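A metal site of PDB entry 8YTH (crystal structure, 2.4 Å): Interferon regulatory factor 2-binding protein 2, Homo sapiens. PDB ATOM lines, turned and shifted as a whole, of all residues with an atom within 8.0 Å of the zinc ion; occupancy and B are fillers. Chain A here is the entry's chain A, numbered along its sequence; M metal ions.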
ATOM      1  N   THR A  12     -16.736   2.094  -4.064  1.00  0.00           N
ATOM      2  CA  THR A  12     -16.821   1.891  -5.504  1.00  0.00           C
ATOM      3  C   THR A  12     -17.966   0.963  -5.891  1.00  0.00           C
ATOM      4  O   THR A  12     -18.095   0.601  -7.066  1.00  0.00           O
ATOM      5  CB  THR A  12     -15.491   1.374  -6.044  1.00  0.00           C
ATOM      6  OG1 THR A  12     -15.551   1.289  -7.472  1.00  0.00           O
ATOM      7  CG2 THR A  12     -15.175   0.000  -5.483  1.00  0.00           C
ATOM      8  N   GLN A  25      -9.786  -0.901   2.200  1.00  0.00           N
ATOM      9  CA  GLN A  25      -8.954  -0.429   1.098  1.00  0.00           C
ATOM     10  C   GLN A  25      -8.186  -1.598   0.509  1.00  0.00           C
ATOM     11  O   GLN A  25      -7.358  -2.209   1.197  1.00  0.00           O
ATOM     12  CB  GLN A  25      -7.982   0.656   1.549  1.00  0.00           C
ATOM     13  CG  GLN A  25      -6.917   0.982   0.520  1.00  0.00           C
ATOM     14  CD  GLN A  25      -7.472   1.686  -0.713  1.00  0.00           C
ATOM     15  OE1 GLN A  25      -7.896   2.845  -0.644  1.00  0.00           O
ATOM     16  NE2 GLN A  25      -7.479   0.992  -1.851  1.00  0.00           N
ATOM     17  N   CYS A  26      -8.474  -1.910  -0.752  1.00  0.00           N
ATOM     18  CA  CYS A  26      -7.722  -2.911  -1.495  1.00  0.00           C
ATOM     19  C   CYS A  26      -6.242  -2.547  -1.501  1.00  0.00           C
ATOM     20  O   CYS A  26      -5.890  -1.396  -1.797  1.00  0.00           O
ATOM     21  CB  CYS A  26      -8.265  -2.994  -2.917  1.00  0.00           C
ATOM     22  SG  CYS A  26      -7.468  -4.108  -4.105  1.00  0.00           S
ATOM     23  N   PRO A  27      -5.337  -3.459  -1.137  1.00  0.00           N
ATOM     24  CA  PRO A  27      -3.914  -3.091  -1.063  1.00  0.00           C
ATOM     25  C   PRO A  27      -3.292  -2.802  -2.417  1.00  0.00           C
ATOM     26  O   PRO A  27      -2.287  -2.081  -2.475  1.00  0.00           O
ATOM     27  CB  PRO A  27      -3.260  -4.311  -0.395  1.00  0.00           C
ATOM     28  CG  PRO A  27      -4.392  -5.024   0.311  1.00  0.00           C
ATOM     29  CD  PRO A  27      -5.578  -4.812  -0.599  1.00  0.00           C
ATOM     30  N   SER A  28      -3.854  -3.320  -3.508  1.00  0.00           N
ATOM     31  CA  SER A  28      -3.288  -3.111  -4.837  1.00  0.00           C
ATOM     32  C   SER A  28      -3.969  -1.976  -5.592  1.00  0.00           C
ATOM     33  O   SER A  28      -3.299  -1.023  -6.005  1.00  0.00           O
ATOM     34  CB  SER A  28      -3.347  -4.413  -5.646  1.00  0.00           C
ATOM     35  OG  SER A  28      -4.379  -5.269  -5.195  1.00  0.00           O
ATOM     36  N   VAL A  29      -5.272  -2.054  -5.805  1.00  0.00           N
ATOM     37  CA  VAL A  29      -6.006  -1.078  -6.620  1.00  0.00           C
ATOM     38  C   VAL A  29      -6.439   0.051  -5.703  1.00  0.00           C
ATOM     39  O   VAL A  29      -7.291  -0.172  -4.812  1.00  0.00           O
ATOM     40  CB  VAL A  29      -7.202  -1.724  -7.326  1.00  0.00           C
ATOM     41  CG1 VAL A  29      -7.915  -0.695  -8.181  1.00  0.00           C
ATOM     42  CG2 VAL A  29      -6.771  -2.921  -8.153  1.00  0.00           C
ATOM     43  N   PRO A  30      -5.917   1.271  -5.871  1.00  0.00           N
ATOM     44  CA  PRO A  30      -6.330   2.367  -4.980  1.00  0.00           C
ATOM     45  C   PRO A  30      -7.809   2.729  -5.080  1.00  0.00           C
ATOM     46  O   PRO A  30      -8.422   3.060  -4.065  1.00  0.00           O
ATOM     47  CB  PRO A  30      -5.429   3.534  -5.420  1.00  0.00           C
ATOM     48  CG  PRO A  30      -4.230   2.881  -6.008  1.00  0.00           C
ATOM     49  CD  PRO A  30      -4.744   1.650  -6.695  1.00  0.00           C
ATOM     50  N   SER A  31      -8.393   2.670  -6.275  1.00  0.00           N
ATOM     51  CA  SER A  31      -9.793   3.057  -6.420  1.00  0.00           C
ATOM     52  C   SER A  31     -10.768   1.982  -5.945  1.00  0.00           C
ATOM     53  O   SER A  31     -11.988   2.159  -6.081  1.00  0.00           O
ATOM     54  CB  SER A  31     -10.097   3.442  -7.884  1.00  0.00           C
ATOM     55  OG  SER A  31      -9.746   2.393  -8.769  1.00  0.00           O
ATOM     56  N   HIS A  32     -10.278   0.882  -5.352  1.00  0.00           N
ATOM     57  CA  HIS A  32     -11.134  -0.126  -4.740  1.00  0.00           C
ATOM     58  C   HIS A  32     -11.319   0.215  -3.254  1.00  0.00           C
ATOM     59  O   HIS A  32     -10.695  -0.373  -2.364  1.00  0.00           O
ATOM     60  CB  HIS A  32     -10.549  -1.524  -4.898  1.00  0.00           C
ATOM     61  CG  HIS A  32     -10.704  -2.132  -6.258  1.00  0.00           C
ATOM     62  ND1 HIS A  32      -9.992  -3.244  -6.645  1.00  0.00           N
ATOM     63  CD2 HIS A  32     -11.498  -1.797  -7.298  1.00  0.00           C
ATOM     64  CE1 HIS A  32     -10.322  -3.558  -7.888  1.00  0.00           C
ATOM     65  NE2 HIS A  32     -11.232  -2.698  -8.312  1.00  0.00           N
ATOM     66  N   LYS A  33     -12.211   1.159  -2.982  1.00  0.00           N
ATOM     67  CA  LYS A  33     -12.673   1.449  -1.634  1.00  0.00           C
ATOM     68  C   LYS A  33     -14.089   0.923  -1.441  1.00  0.00           C
ATOM     69  O   LYS A  33     -14.913   0.980  -2.359  1.00  0.00           O
ATOM     70  CB  LYS A  33     -12.635   2.958  -1.338  1.00  0.00           C
ATOM     71  CG  LYS A  33     -11.223   3.489  -1.195  1.00  0.00           C
ATOM     72  CD  LYS A  33     -11.216   4.987  -1.003  1.00  0.00           C
ATOM     73  CE  LYS A  33     -10.174   5.609  -1.901  1.00  0.00           C
ATOM     74  NZ  LYS A  33      -8.851   4.949  -1.725  1.00  0.00           N
ATOM     75  N   PHE A  34     -14.359   0.388  -0.243  1.00  0.00           N
ATOM     76  CA  PHE A  34     -15.625  -0.247   0.057  1.00  0.00           C
ATOM     77  C   PHE A  34     -16.069   0.131   1.461  1.00  0.00           C
ATOM     78  O   PHE A  34     -15.281   0.041   2.402  1.00  0.00           O
ATOM     79  CB  PHE A  34     -15.528  -1.778  -0.046  1.00  0.00           C
ATOM     80  CG  PHE A  34     -14.774  -2.274  -1.249  1.00  0.00           C
ATOM     81  CD1 PHE A  34     -15.395  -2.386  -2.485  1.00  0.00           C
ATOM     82  CD2 PHE A  34     -13.439  -2.640  -1.133  1.00  0.00           C
ATOM     83  CE1 PHE A  34     -14.695  -2.849  -3.592  1.00  0.00           C
ATOM     84  CE2 PHE A  34     -12.730  -3.101  -2.240  1.00  0.00           C
ATOM     85  CZ  PHE A  34     -13.365  -3.198  -3.463  1.00  0.00           C
ATOM     86  N   TYR A  53     -11.941 -12.685  -1.072  1.00  0.00           N
ATOM     87  CA  TYR A  53     -10.979 -11.857  -1.763  1.00  0.00           C
ATOM     88  C   TYR A  53     -11.553 -10.452  -1.940  1.00  0.00           C
ATOM     89  O   TYR A  53     -12.533 -10.073  -1.272  1.00  0.00           O
ATOM     90  CB  TYR A  53     -10.592 -12.510  -3.095  1.00  0.00           C
ATOM     91  N   CYS A  54     -10.959  -9.665  -2.831  1.00  0.00           N
ATOM     92  CA  CYS A  54     -11.303  -8.248  -2.948  1.00  0.00           C
ATOM     93  C   CYS A  54     -12.781  -8.092  -3.308  1.00  0.00           C
ATOM     94  O   CYS A  54     -13.239  -8.700  -4.281  1.00  0.00           O
ATOM     95  CB  CYS A  54     -10.439  -7.570  -3.993  1.00  0.00           C
ATOM     96  SG  CYS A  54     -10.878  -5.835  -4.210  1.00  0.00           S
ATOM     97  N   PRO A  55     -13.543  -7.280  -2.568  1.00  0.00           N
ATOM     98  CA  PRO A  55     -14.978  -7.143  -2.879  1.00  0.00           C
ATOM     99  C   PRO A  55     -15.228  -6.653  -4.283  1.00  0.00           C
ATOM    100  O   PRO A  55     -16.353  -6.798  -4.778  1.00  0.00           O
ATOM    101  CB  PRO A  55     -15.475  -6.135  -1.833  1.00  0.00           C
ATOM    102  CG  PRO A  55     -14.493  -6.229  -0.725  1.00  0.00           C
ATOM    103  CD  PRO A  55     -13.172  -6.477  -1.391  1.00  0.00           C
ATOM    104  N   SER A  56     -14.227  -6.097  -4.970  1.00  0.00           N
ATOM    105  CA  SER A  56     -14.408  -5.738  -6.365  1.00  0.00           C
ATOM    106  C   SER A  56     -14.641  -6.977  -7.228  1.00  0.00           C
ATOM    107  O   SER A  56     -15.261  -6.868  -8.293  1.00  0.00           O
ATOM    108  CB  SER A  56     -13.199  -4.964  -6.885  1.00  0.00           C
ATOM    109  OG  SER A  56     -13.518  -4.226  -8.065  1.00  0.00           O
ATOM    110  N   GLY A  57     -14.179  -8.141  -6.789  1.00  0.00           N
ATOM    111  CA  GLY A  57     -14.302  -9.349  -7.563  1.00  0.00           C
ATOM    112  C   GLY A  57     -13.178  -9.591  -8.538  1.00  0.00           C
ATOM    113  O   GLY A  57     -13.095 -10.681  -9.113  1.00  0.00           O
ATOM    114  N   GLU A  58     -12.304  -8.606  -8.737  1.00  0.00           N
ATOM    115  CA  GLU A  58     -11.135  -8.763  -9.594  1.00  0.00           C
ATOM    116  C   GLU A  58     -10.031  -9.595  -8.947  1.00  0.00           C
ATOM    117  O   GLU A  58      -8.966  -9.725  -9.549  1.00  0.00           O
ATOM    118  CB  GLU A  58     -10.567  -7.402  -9.980  1.00  0.00           C
ATOM    119  N   LYS A  59     -10.260 -10.132  -7.738  1.00  0.00           N
ATOM    120  CA  LYS A  59      -9.291 -10.938  -6.998  1.00  0.00           C
ATOM    121  C   LYS A  59      -7.896 -10.315  -7.052  1.00  0.00           C
ATOM    122  O   LYS A  59      -6.924 -10.905  -7.524  1.00  0.00           O
ATOM    123  CB  LYS A  59      -9.257 -12.382  -7.514  1.00  0.00           C
ATOM    124  N   CYS A  60      -7.810  -9.094  -6.521  1.00  0.00           N
ATOM    125  CA  CYS A  60      -6.599  -8.322  -6.605  1.00  0.00           C
ATOM    126  C   CYS A  60      -5.505  -8.907  -5.702  1.00  0.00           C
ATOM    127  O   CYS A  60      -5.807  -9.526  -4.671  1.00  0.00           O
ATOM    128  CB  CYS A  60      -6.902  -6.874  -6.228  1.00  0.00           C
ATOM    129  SG  CYS A  60      -8.440  -6.322  -6.988  1.00  0.00           S
ATOM    130  N   PRO A  61      -4.242  -8.750  -6.075  1.00  0.00           N
ATOM    131  CA  PRO A  61      -3.152  -9.401  -5.346  1.00  0.00           C
ATOM    132  C   PRO A  61      -2.525  -8.520  -4.280  1.00  0.00           C
ATOM    133  O   PRO A  61      -2.895  -7.356  -4.107  1.00  0.00           O
ATOM    134  CB  PRO A  61      -2.148  -9.711  -6.448  1.00  0.00           C
ATOM    135  CG  PRO A  61      -2.303  -8.540  -7.375  1.00  0.00           C
ATOM    136  CD  PRO A  61      -3.774  -8.158  -7.339  1.00  0.00           C
ATOM    137  N   TRP A  69      -4.992 -11.158  -2.445  1.00  0.00           N
ATOM    138  CA  TRP A  69      -5.157 -10.885  -1.021  1.00  0.00           C
ATOM    139  C   TRP A  69      -6.534 -11.345  -0.552  1.00  0.00           C
ATOM    140  O   TRP A  69      -7.495 -11.407  -1.321  1.00  0.00           O
ATOM    141  CB  TRP A  69      -4.960  -9.402  -0.725  1.00  0.00           C
ATOM    142  CG  TRP A  69      -6.079  -8.477  -1.144  1.00  0.00           C
ATOM    143  CD1 TRP A  69      -6.162  -7.750  -2.298  1.00  0.00           C
ATOM    144  CD2 TRP A  69      -7.259  -8.149  -0.388  1.00  0.00           C
ATOM    145  NE1 TRP A  69      -7.317  -7.015  -2.324  1.00  0.00           N
ATOM    146  CE2 TRP A  69      -8.011  -7.247  -1.156  1.00  0.00           C
ATOM    147  CE3 TRP A  69      -7.755  -8.557   0.856  1.00  0.00           C
ATOM    148  CZ2 TRP A  69      -9.232  -6.729  -0.724  1.00  0.00           C
ATOM    149  CZ3 TRP A  69      -8.964  -8.046   1.287  1.00  0.00           C
ATOM    150  CH2 TRP A  69      -9.696  -7.135   0.492  1.00  0.00           C
HETATM  151 ZN    ZN M   1      -9.227  -4.797  -5.453  1.00  0.00          ZN
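A ring nitrogen (NE2) of His 32 is in hydrogen-bond range of the side-chain hydroxyl (OG) of Ser 56 (2.8 Å).
The backbone carbonyl oxygen (O) of Cys 60 sits at hydrogen-bond distance from the backbone NH (N) of Trp 69 (2.9 Å).
The side-chain sulfur (SG) of Cys 54 lies close to the backbone NH (N) of Ser 56.
N of Val 29 sits close to SG of Cys 26, 3.5 Å away.
The indole nitrogen of Trp 69 lies close to the side-chain sulfur of Cys 26 (3.4 Å).
SG of Cys 26 lies close to OG of Ser 28 (3.5 Å).
The nearest printed residue that does not touch the zinc ion is Val 29 (4.1 Å).
ND1 of His 32 is bound to the zinc ion, 2.1 Å away.
The side-chain sulfur (SG) of Cys 60 binds the zinc ion (2.3 Å).
SG of Cys 54 is bound to the zinc ion, at 2.3 Å.
The zinc ion is bound by SG of Cys 26, at 2.3 Å.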
